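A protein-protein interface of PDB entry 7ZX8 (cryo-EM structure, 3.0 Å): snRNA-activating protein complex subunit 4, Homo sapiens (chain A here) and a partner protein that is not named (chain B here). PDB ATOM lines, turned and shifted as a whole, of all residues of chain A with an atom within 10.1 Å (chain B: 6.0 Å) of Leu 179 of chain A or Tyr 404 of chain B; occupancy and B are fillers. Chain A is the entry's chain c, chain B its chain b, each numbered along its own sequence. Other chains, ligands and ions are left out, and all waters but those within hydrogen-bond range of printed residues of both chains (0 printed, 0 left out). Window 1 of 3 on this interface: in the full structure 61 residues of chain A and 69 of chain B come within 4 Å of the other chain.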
ATOM      1  N   ILE A 173       4.717  37.161   6.022  1.00  0.00           N
ATOM      2  CA  ILE A 173       3.696  36.312   6.626  1.00  0.00           C
ATOM      3  C   ILE A 173       2.526  36.280   5.657  1.00  0.00           C
ATOM      4  O   ILE A 173       2.353  37.201   4.853  1.00  0.00           O
ATOM      5  CB  ILE A 173       3.257  36.814   8.012  1.00  0.00           C
ATOM      6  CG1 ILE A 173       2.999  35.640   8.951  1.00  0.00           C
ATOM      7  CG2 ILE A 173       2.014  37.682   7.905  1.00  0.00           C
ATOM      8  CD1 ILE A 173       4.259  34.959   9.414  1.00  0.00           C
ATOM      9  N   LYS A 174       1.727  35.229   5.707  1.00  0.00           N
ATOM     10  CA  LYS A 174       0.505  35.199   4.923  1.00  0.00           C
ATOM     11  C   LYS A 174      -0.705  35.284   5.838  1.00  0.00           C
ATOM     12  O   LYS A 174      -1.041  34.343   6.555  1.00  0.00           O
ATOM     13  CB  LYS A 174       0.433  33.932   4.068  1.00  0.00           C
ATOM     14  CG  LYS A 174       1.594  33.777   3.110  1.00  0.00           C
ATOM     15  CD  LYS A 174       1.671  34.943   2.146  1.00  0.00           C
ATOM     16  CE  LYS A 174       0.553  34.880   1.126  1.00  0.00           C
ATOM     17  NZ  LYS A 174       0.727  35.895   0.054  1.00  0.00           N
ATOM     18  N   ALA A 175      -1.364  36.434   5.800  1.00  0.00           N
ATOM     19  CA  ALA A 175      -2.602  36.609   6.540  1.00  0.00           C
ATOM     20  C   ALA A 175      -3.665  35.669   5.986  1.00  0.00           C
ATOM     21  O   ALA A 175      -3.525  35.106   4.899  1.00  0.00           O
ATOM     22  CB  ALA A 175      -3.081  38.058   6.467  1.00  0.00           C
ATOM     23  N   PHE A 176      -4.735  35.494   6.758  1.00  0.00           N
ATOM     24  CA  PHE A 176      -5.764  34.545   6.356  1.00  0.00           C
ATOM     25  C   PHE A 176      -6.448  34.986   5.071  1.00  0.00           C
ATOM     26  O   PHE A 176      -6.713  34.164   4.187  1.00  0.00           O
ATOM     27  CB  PHE A 176      -6.779  34.368   7.479  1.00  0.00           C
ATOM     28  CG  PHE A 176      -6.365  33.363   8.506  1.00  0.00           C
ATOM     29  CD1 PHE A 176      -5.806  32.157   8.122  1.00  0.00           C
ATOM     30  CD2 PHE A 176      -6.525  33.625   9.853  1.00  0.00           C
ATOM     31  CE1 PHE A 176      -5.421  31.230   9.066  1.00  0.00           C
ATOM     32  CE2 PHE A 176      -6.140  32.701  10.797  1.00  0.00           C
ATOM     33  CZ  PHE A 176      -5.590  31.506  10.400  1.00  0.00           C
ATOM     34  N   GLU A 177      -6.728  36.281   4.944  1.00  0.00           N
ATOM     35  CA  GLU A 177      -7.351  36.793   3.734  1.00  0.00           C
ATOM     36  C   GLU A 177      -6.489  36.589   2.497  1.00  0.00           C
ATOM     37  O   GLU A 177      -7.028  36.271   1.433  1.00  0.00           O
ATOM     38  CB  GLU A 177      -7.666  38.278   3.894  1.00  0.00           C
ATOM     39  CG  GLU A 177      -8.946  38.555   4.650  1.00  0.00           C
ATOM     40  CD  GLU A 177      -8.767  38.471   6.150  1.00  0.00           C
ATOM     41  OE1 GLU A 177      -7.640  38.172   6.596  1.00  0.00           O
ATOM     42  OE2 GLU A 177      -9.750  38.707   6.879  1.00  0.00           O
ATOM     43  N   GLU A 178      -5.177  36.750   2.611  1.00  0.00           N
ATOM     44  CA  GLU A 178      -4.294  36.619   1.466  1.00  0.00           C
ATOM     45  C   GLU A 178      -4.145  35.182   0.989  1.00  0.00           C
ATOM     46  O   GLU A 178      -3.569  34.959  -0.079  1.00  0.00           O
ATOM     47  CB  GLU A 178      -2.916  37.191   1.797  1.00  0.00           C
ATOM     48  CG  GLU A 178      -2.972  38.495   2.570  1.00  0.00           C
ATOM     49  CD  GLU A 178      -1.626  39.184   2.654  1.00  0.00           C
ATOM     50  OE1 GLU A 178      -0.915  39.235   1.629  1.00  0.00           O
ATOM     51  OE2 GLU A 178      -1.277  39.670   3.748  1.00  0.00           O
ATOM     52  N   LEU A 179      -4.648  34.214   1.745  1.00  0.00           N
ATOM     53  CA  LEU A 179      -4.532  32.816   1.370  1.00  0.00           C
ATOM     54  C   LEU A 179      -5.798  32.254   0.748  1.00  0.00           C
ATOM     55  O   LEU A 179      -5.797  31.100   0.313  1.00  0.00           O
ATOM     56  CB  LEU A 179      -4.164  31.981   2.596  1.00  0.00           C
ATOM     57  CG  LEU A 179      -2.781  32.253   3.175  1.00  0.00           C
ATOM     58  CD1 LEU A 179      -2.743  31.859   4.637  1.00  0.00           C
ATOM     59  CD2 LEU A 179      -1.736  31.491   2.386  1.00  0.00           C
ATOM     60  N   LEU A 180      -6.872  33.036   0.697  1.00  0.00           N
ATOM     61  CA  LEU A 180      -8.141  32.541   0.186  1.00  0.00           C
ATOM     62  C   LEU A 180      -8.015  32.218  -1.296  1.00  0.00           C
ATOM     63  O   LEU A 180      -7.573  33.058  -2.085  1.00  0.00           O
ATOM     64  CB  LEU A 180      -9.238  33.570   0.422  1.00  0.00           C
ATOM     65  CG  LEU A 180      -9.368  34.084   1.853  1.00  0.00           C
ATOM     66  CD1 LEU A 180     -10.604  34.939   1.997  1.00  0.00           C
ATOM     67  CD2 LEU A 180      -9.406  32.929   2.825  1.00  0.00           C
ATOM     68  N   VAL A 181      -8.399  31.003  -1.674  1.00  0.00           N
ATOM     69  CA  VAL A 181      -8.403  30.575  -3.064  1.00  0.00           C
ATOM     70  C   VAL A 181      -9.840  30.264  -3.459  1.00  0.00           C
ATOM     71  O   VAL A 181     -10.477  29.373  -2.882  1.00  0.00           O
ATOM     72  CB  VAL A 181      -7.472  29.373  -3.303  1.00  0.00           C
ATOM     73  CG1 VAL A 181      -7.830  28.190  -2.418  1.00  0.00           C
ATOM     74  CG2 VAL A 181      -7.518  28.963  -4.755  1.00  0.00           C
ATOM     75  N   THR A 182     -10.341  30.984  -4.468  1.00  0.00           N
ATOM     76  CA  THR A 182     -11.701  30.700  -4.996  1.00  0.00           C
ATOM     77  C   THR A 182     -11.546  30.050  -6.376  1.00  0.00           C
ATOM     78  O   THR A 182     -10.801  30.608  -7.206  1.00  0.00           O
ATOM     79  CB  THR A 182     -12.542  31.981  -5.076  1.00  0.00           C
ATOM     80  OG1 THR A 182     -11.881  32.899  -5.947  1.00  0.00           O
ATOM     81  CG2 THR A 182     -12.762  32.625  -3.725  1.00  0.00           C
ATOM     82  N   LYS A 183     -12.213  28.915  -6.603  1.00  0.00           N
ATOM     83  CA  LYS A 183     -12.149  28.239  -7.926  1.00  0.00           C
ATOM     84  C   LYS A 183     -12.739  29.187  -8.975  1.00  0.00           C
ATOM     85  O   LYS A 183     -13.784  29.809  -8.693  1.00  0.00           O
ATOM     86  CB  LYS A 183     -12.883  26.895  -7.866  1.00  0.00           C
ATOM     87  CG  LYS A 183     -13.657  26.499  -9.118  1.00  0.00           C
ATOM     88  CD  LYS A 183     -15.103  26.143  -8.841  1.00  0.00           C
ATOM     89  CE  LYS A 183     -16.082  27.151  -9.404  1.00  0.00           C
ATOM     90  NZ  LYS A 183     -16.644  28.020  -8.344  1.00  0.00           N
ATOM     91  N   SER A 276      -7.907  40.178  -7.288  1.00  0.00           N
ATOM     92  CA  SER A 276      -6.780  41.093  -7.274  1.00  0.00           C
ATOM     93  C   SER A 276      -6.146  41.175  -8.653  1.00  0.00           C
ATOM     94  O   SER A 276      -6.279  40.272  -9.485  1.00  0.00           O
ATOM     95  CB  SER A 276      -5.739  40.650  -6.250  1.00  0.00           C
ATOM     96  OG  SER A 276      -5.013  39.536  -6.729  1.00  0.00           O
ATOM     97  N   GLU A 279      -3.576  38.418  -9.369  1.00  0.00           N
ATOM     98  CA  GLU A 279      -4.255  37.144  -9.565  1.00  0.00           C
ATOM     99  C   GLU A 279      -4.741  37.003 -10.994  1.00  0.00           C
ATOM    100  O   GLU A 279      -4.500  35.980 -11.646  1.00  0.00           O
ATOM    101  CB  GLU A 279      -5.420  37.025  -8.588  1.00  0.00           C
ATOM    102  CG  GLU A 279      -6.061  35.661  -8.546  1.00  0.00           C
ATOM    103  CD  GLU A 279      -6.950  35.487  -7.336  1.00  0.00           C
ATOM    104  OE1 GLU A 279      -7.202  36.491  -6.637  1.00  0.00           O
ATOM    105  OE2 GLU A 279      -7.398  34.352  -7.081  1.00  0.00           O
ATOM    106  N   TYR A 377      -0.838  13.632   6.231  1.00  0.00           N
ATOM    107  CA  TYR A 377      -0.003  14.821   6.141  1.00  0.00           C
ATOM    108  C   TYR A 377       1.150  14.754   7.134  1.00  0.00           C
ATOM    109  O   TYR A 377       1.883  15.734   7.309  1.00  0.00           O
ATOM    110  CB  TYR A 377      -0.846  16.081   6.348  1.00  0.00           C
ATOM    111  CG  TYR A 377      -2.061  16.198   5.427  1.00  0.00           C
ATOM    112  CD1 TYR A 377      -3.052  17.136   5.678  1.00  0.00           C
ATOM    113  CD2 TYR A 377      -2.216  15.378   4.309  1.00  0.00           C
ATOM    114  CE1 TYR A 377      -4.163  17.257   4.860  1.00  0.00           C
ATOM    115  CE2 TYR A 377      -3.330  15.490   3.479  1.00  0.00           C
ATOM    116  CZ  TYR A 377      -4.298  16.434   3.761  1.00  0.00           C
ATOM    117  OH  TYR A 377      -5.399  16.558   2.947  1.00  0.00           O
ATOM    118  N   TYR A 378       1.321  13.609   7.802  1.00  0.00           N
ATOM    119  CA  TYR A 378       2.510  13.328   8.599  1.00  0.00           C
ATOM    120  C   TYR A 378       3.302  12.169   8.010  1.00  0.00           C
ATOM    121  O   TYR A 378       4.368  11.823   8.523  1.00  0.00           O
ATOM    122  CB  TYR A 378       2.144  12.996  10.042  1.00  0.00           C
ATOM    123  CG  TYR A 378       1.762  14.181  10.877  1.00  0.00           C
ATOM    124  CD1 TYR A 378       1.211  14.009  12.132  1.00  0.00           C
ATOM    125  CD2 TYR A 378       1.942  15.469  10.417  1.00  0.00           C
ATOM    126  CE1 TYR A 378       0.854  15.086  12.909  1.00  0.00           C
ATOM    127  CE2 TYR A 378       1.586  16.556  11.186  1.00  0.00           C
ATOM    128  CZ  TYR A 378       1.042  16.355  12.434  1.00  0.00           C
ATOM    129  OH  TYR A 378       0.680  17.425  13.216  1.00  0.00           O
ATOM    130  N   GLN B 226       2.845  28.722  11.399  1.00  0.00           N
ATOM    131  CA  GLN B 226       3.189  29.563  10.261  1.00  0.00           C
ATOM    132  C   GLN B 226       4.544  30.220  10.454  1.00  0.00           C
ATOM    133  O   GLN B 226       4.632  31.429  10.695  1.00  0.00           O
ATOM    134  CB  GLN B 226       2.120  30.634  10.030  1.00  0.00           C
ATOM    135  CG  GLN B 226       0.835  30.109   9.454  1.00  0.00           C
ATOM    136  CD  GLN B 226      -0.218  31.178   9.348  1.00  0.00           C
ATOM    137  OE1 GLN B 226      -0.217  32.143  10.112  1.00  0.00           O
ATOM    138  NE2 GLN B 226      -1.130  31.020   8.397  1.00  0.00           N
ATOM    139  N   ARG B 352      -6.362  21.887   2.296  1.00  0.00           N
ATOM    140  CA  ARG B 352      -5.883  22.381   1.011  1.00  0.00           C
ATOM    141  C   ARG B 352      -4.864  21.401   0.455  1.00  0.00           C
ATOM    142  O   ARG B 352      -3.805  21.197   1.049  1.00  0.00           O
ATOM    143  CB  ARG B 352      -5.258  23.759   1.177  1.00  0.00           C
ATOM    144  CG  ARG B 352      -6.238  24.850   1.501  1.00  0.00           C
ATOM    145  CD  ARG B 352      -6.603  25.656   0.277  1.00  0.00           C
ATOM    146  NE  ARG B 352      -7.717  26.558   0.542  1.00  0.00           N
ATOM    147  CZ  ARG B 352      -7.649  27.631   1.324  1.00  0.00           C
ATOM    148  NH1 ARG B 352      -6.517  27.954   1.933  1.00  0.00           N
ATOM    149  NH2 ARG B 352      -8.724  28.386   1.501  1.00  0.00           N
ATOM    150  N   ALA B 362      -0.920  20.791   1.057  1.00  0.00           N
ATOM    151  CA  ALA B 362      -0.221  21.991   0.612  1.00  0.00           C
ATOM    152  C   ALA B 362       0.811  22.385   1.652  1.00  0.00           C
ATOM    153  O   ALA B 362       0.499  23.005   2.667  1.00  0.00           O
ATOM    154  CB  ALA B 362      -1.210  23.121   0.375  1.00  0.00           C
ATOM    155  N   ARG B 363       2.064  22.031   1.390  1.00  0.00           N
ATOM    156  CA  ARG B 363       3.157  22.466   2.245  1.00  0.00           C
ATOM    157  C   ARG B 363       3.714  23.828   1.848  1.00  0.00           C
ATOM    158  O   ARG B 363       4.324  24.493   2.689  1.00  0.00           O
ATOM    159  CB  ARG B 363       4.275  21.424   2.221  1.00  0.00           C
ATOM    160  CG  ARG B 363       3.932  20.092   2.886  1.00  0.00           C
ATOM    161  CD  ARG B 363       4.477  19.988   4.306  1.00  0.00           C
ATOM    162  NE  ARG B 363       3.525  20.393   5.340  1.00  0.00           N
ATOM    163  CZ  ARG B 363       2.692  19.562   5.966  1.00  0.00           C
ATOM    164  NH1 ARG B 363       2.690  18.270   5.673  1.00  0.00           N
ATOM    165  NH2 ARG B 363       1.869  20.021   6.898  1.00  0.00           N
ATOM    166  N   TRP B 364       3.504  24.272   0.608  1.00  0.00           N
ATOM    167  CA  TRP B 364       4.141  25.488   0.112  1.00  0.00           C
ATOM    168  C   TRP B 364       3.110  26.371  -0.571  1.00  0.00           C
ATOM    169  O   TRP B 364       2.321  25.877  -1.380  1.00  0.00           O
ATOM    170  CB  TRP B 364       5.253  25.145  -0.867  1.00  0.00           C
ATOM    171  CG  TRP B 364       6.399  24.468  -0.243  1.00  0.00           C
ATOM    172  CD1 TRP B 364       6.765  23.167  -0.394  1.00  0.00           C
ATOM    173  CD2 TRP B 364       7.354  25.054   0.639  1.00  0.00           C
ATOM    174  NE1 TRP B 364       7.890  22.906   0.342  1.00  0.00           N
ATOM    175  CE2 TRP B 364       8.271  24.051   0.985  1.00  0.00           C
ATOM    176  CE3 TRP B 364       7.520  26.333   1.171  1.00  0.00           C
ATOM    177  CZ2 TRP B 364       9.335  24.284   1.841  1.00  0.00           C
ATOM    178  CZ3 TRP B 364       8.576  26.563   2.014  1.00  0.00           C
ATOM    179  CH2 TRP B 364       9.473  25.549   2.342  1.00  0.00           C
ATOM    180  N   VAL B 365       3.121  27.666  -0.271  1.00  0.00           N
ATOM    181  CA  VAL B 365       2.278  28.634  -0.966  1.00  0.00           C
ATOM    182  C   VAL B 365       3.172  29.589  -1.738  1.00  0.00           C
ATOM    183  O   VAL B 365       4.064  30.221  -1.161  1.00  0.00           O
ATOM    184  CB  VAL B 365       1.373  29.401   0.012  1.00  0.00           C
ATOM    185  CG1 VAL B 365       2.166  29.924   1.185  1.00  0.00           C
ATOM    186  CG2 VAL B 365       0.704  30.550  -0.700  1.00  0.00           C
ATOM    187  N   PRO B 376      -1.948  32.824  -5.724  1.00  0.00           N
ATOM    188  CA  PRO B 376      -1.522  32.050  -4.559  1.00  0.00           C
ATOM    189  C   PRO B 376      -1.743  30.587  -4.859  1.00  0.00           C
ATOM    190  O   PRO B 376      -2.878  30.107  -4.817  1.00  0.00           O
ATOM    191  CB  PRO B 376      -2.419  32.564  -3.430  1.00  0.00           C
ATOM    192  CG  PRO B 376      -3.584  33.207  -4.107  1.00  0.00           C
ATOM    193  CD  PRO B 376      -3.360  33.214  -5.594  1.00  0.00           C
ATOM    194  N   PHE B 378      -0.864  26.526  -4.231  1.00  0.00           N
ATOM    195  CA  PHE B 378      -0.492  25.630  -3.150  1.00  0.00           C
ATOM    196  C   PHE B 378       0.109  24.364  -3.737  1.00  0.00           C
ATOM    197  O   PHE B 378      -0.553  23.651  -4.497  1.00  0.00           O
ATOM    198  CB  PHE B 378      -1.711  25.309  -2.296  1.00  0.00           C
ATOM    199  CG  PHE B 378      -2.335  26.511  -1.664  1.00  0.00           C
ATOM    200  CD1 PHE B 378      -1.571  27.408  -0.951  1.00  0.00           C
ATOM    201  CD2 PHE B 378      -3.686  26.755  -1.794  1.00  0.00           C
ATOM    202  CE1 PHE B 378      -2.145  28.515  -0.367  1.00  0.00           C
ATOM    203  CE2 PHE B 378      -4.258  27.864  -1.214  1.00  0.00           C
ATOM    204  CZ  PHE B 378      -3.487  28.745  -0.501  1.00  0.00           C
ATOM    205  N   TYR B 402       6.454  30.705   0.336  1.00  0.00           N
ATOM    206  CA  TYR B 402       6.301  30.729   1.774  1.00  0.00           C
ATOM    207  C   TYR B 402       5.865  29.360   2.278  1.00  0.00           C
ATOM    208  O   TYR B 402       5.219  28.597   1.552  1.00  0.00           O
ATOM    209  CB  TYR B 402       5.266  31.770   2.196  1.00  0.00           C
ATOM    210  CG  TYR B 402       5.444  33.119   1.555  1.00  0.00           C
ATOM    211  CD1 TYR B 402       5.991  34.175   2.263  1.00  0.00           C
ATOM    212  CD2 TYR B 402       5.048  33.344   0.249  1.00  0.00           C
ATOM    213  CE1 TYR B 402       6.150  35.414   1.681  1.00  0.00           C
ATOM    214  CE2 TYR B 402       5.205  34.575  -0.342  1.00  0.00           C
ATOM    215  CZ  TYR B 402       5.756  35.606   0.377  1.00  0.00           C
ATOM    216  OH  TYR B 402       5.911  36.836  -0.212  1.00  0.00           O
ATOM    217  N   PRO B 403       6.209  29.012   3.511  1.00  0.00           N
ATOM    218  CA  PRO B 403       5.751  27.739   4.058  1.00  0.00           C
ATOM    219  C   PRO B 403       4.277  27.820   4.402  1.00  0.00           C
ATOM    220  O   PRO B 403       3.805  28.797   4.987  1.00  0.00           O
ATOM    221  CB  PRO B 403       6.605  27.558   5.319  1.00  0.00           C
ATOM    222  CG  PRO B 403       7.588  28.681   5.310  1.00  0.00           C
ATOM    223  CD  PRO B 403       6.994  29.765   4.491  1.00  0.00           C
ATOM    224  N   TYR B 404       3.545  26.777   4.034  1.00  0.00           N
ATOM    225  CA  TYR B 404       2.124  26.713   4.319  1.00  0.00           C
ATOM    226  C   TYR B 404       1.867  25.649   5.369  1.00  0.00           C
ATOM    227  O   TYR B 404       2.444  24.559   5.321  1.00  0.00           O
ATOM    228  CB  TYR B 404       1.308  26.410   3.075  1.00  0.00           C
ATOM    229  CG  TYR B 404      -0.163  26.633   3.289  1.00  0.00           C
ATOM    230  CD1 TYR B 404      -0.608  27.730   4.009  1.00  0.00           C
ATOM    231  CD2 TYR B 404      -1.104  25.763   2.773  1.00  0.00           C
ATOM    232  CE1 TYR B 404      -1.945  27.949   4.212  1.00  0.00           C
ATOM    233  CE2 TYR B 404      -2.443  25.976   2.971  1.00  0.00           C
ATOM    234  CZ  TYR B 404      -2.859  27.071   3.691  1.00  0.00           C
ATOM    235  OH  TYR B 404      -4.199  27.294   3.893  1.00  0.00           O
ATOM    236  N   VAL B 405       0.991  25.973   6.315  1.00  0.00           N
ATOM    237  CA  VAL B 405       0.667  25.065   7.400  1.00  0.00           C
ATOM    238  C   VAL B 405      -0.588  24.248   7.139  1.00  0.00           C
ATOM    239  O   VAL B 405      -0.782  23.226   7.809  1.00  0.00           O
ATOM    240  CB  VAL B 405       0.528  25.830   8.727  1.00  0.00           C
ATOM    241  CG1 VAL B 405       1.871  26.353   9.156  1.00  0.00           C
ATOM    242  CG2 VAL B 405      -0.453  26.955   8.554  1.00  0.00           C
ATOM    243  N   ASP B 406      -1.440  24.657   6.196  1.00  0.00           N
ATOM    244  CA  ASP B 406      -2.632  23.899   5.835  1.00  0.00           C
ATOM    245  C   ASP B 406      -3.520  23.710   7.058  1.00  0.00           C
ATOM    246  O   ASP B 406      -3.602  22.606   7.605  1.00  0.00           O
ATOM    247  CB  ASP B 406      -2.234  22.552   5.226  1.00  0.00           C
ATOM    248  CG  ASP B 406      -3.424  21.713   4.841  1.00  0.00           C
ATOM    249  OD1 ASP B 406      -4.323  22.236   4.154  1.00  0.00           O
ATOM    250  OD2 ASP B 406      -3.450  20.519   5.202  1.00  0.00           O
ATOM    251  N   PRO B 407      -4.203  24.762   7.511  1.00  0.00           N
ATOM    252  CA  PRO B 407      -4.886  24.719   8.807  1.00  0.00           C
ATOM    253  C   PRO B 407      -5.944  23.641   8.922  1.00  0.00           C
ATOM    254  O   PRO B 407      -6.413  23.377  10.036  1.00  0.00           O
ATOM    255  CB  PRO B 407      -5.517  26.108   8.896  1.00  0.00           C
ATOM    256  CG  PRO B 407      -5.776  26.460   7.493  1.00  0.00           C
ATOM    257  CD  PRO B 407      -4.610  25.933   6.724  1.00  0.00           C
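O of Tyr 377 of chain A lies within hydrogen-bond range of NH1 of Arg 363 of chain B, 3.1 Å away.
N of Ala 362 of chain B lies within hydrogen-bond range of O of Arg 352 of chain B (2.9 Å).
NH1 of Arg 352 of chain B lies within hydrogen-bond range of OH of Tyr 404 of chain B.
The side-chain carboxylate (OD1) of Asp 406 of chain B lies within hydrogen-bond range of the backbone NH (N) of Arg 352 of chain B (2.8 Å).
The backbone NH of Tyr 404 of chain B lies within hydrogen-bond range of the backbone carbonyl oxygen of Arg 363 of chain B (2.8 Å).
Among the printed residues, merely in contact across the chains: Tyr 377 of chain A with Asp 406 of chain B, Val 181 of chain A with Arg 352 of chain B, Leu 179 of chain A with Phe 378 of chain B, Leu 179 of chain A with Arg 352 of chain B, Ile 173 of chain A with Gln 226 of chain B, Val 181 of chain A with Phe 378 of chain B, Lys 174 of chain A with Gln 226 of chain B and Leu 179 of chain A with Tyr 404 of chain B.
Of the printed residues of chain B, Leu 179 of chain A touches Arg 352 (3.6 Å), Phe 378 (3.4 Å) and Tyr 404 (3.99 Å).
Printed residues of chain A within 4 Å of Tyr 404 of chain B: Leu 179.
No residue of chain A comes within 4 Å of Ala 362 of chain B.
Pro 403 of chain B touches none of the printed residues of chain A.
Asp 406 of chain B touches one residue of chain A.
Of the printed residues of chain B, Lys 174 of chain A touches Gln 226 (3.8 Å).
Of the printed residues of chain A, Arg 363 of chain B touches Tyr 377.
Printed residues of chain A within 4 Å of Phe 378 of chain B: Leu 179 (3.4 Å) and Val 181 (3.8 Å).
Of the printed residues of chain B, Val 181 of chain A touches Arg 352 (3.4 Å) and Phe 378 (3.8 Å).
Tyr 378 of chain A touches none of the printed residues of chain B.
Pro 407 of chain B touches none of the printed residues of chain A.
The nearest printed residue of chain A that does not touch Tyr 404 of chain B is Lys 174 of chain A (6.3 Å).
The nearest printed residue of chain A that does not touch Phe 378 of chain B is Leu 180 of chain A (5.6 Å).
Hydrophobic or aromatic side chains of chain A that line the printed part of chain B: Ile 173, Leu 179, Val 181 and Tyr 377.
Hydrophobic or aromatic side chains of chain B that line the printed part of chain A: Phe 378 and Tyr 404.
Among the printed residues, 9 pairs touch across the chains.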
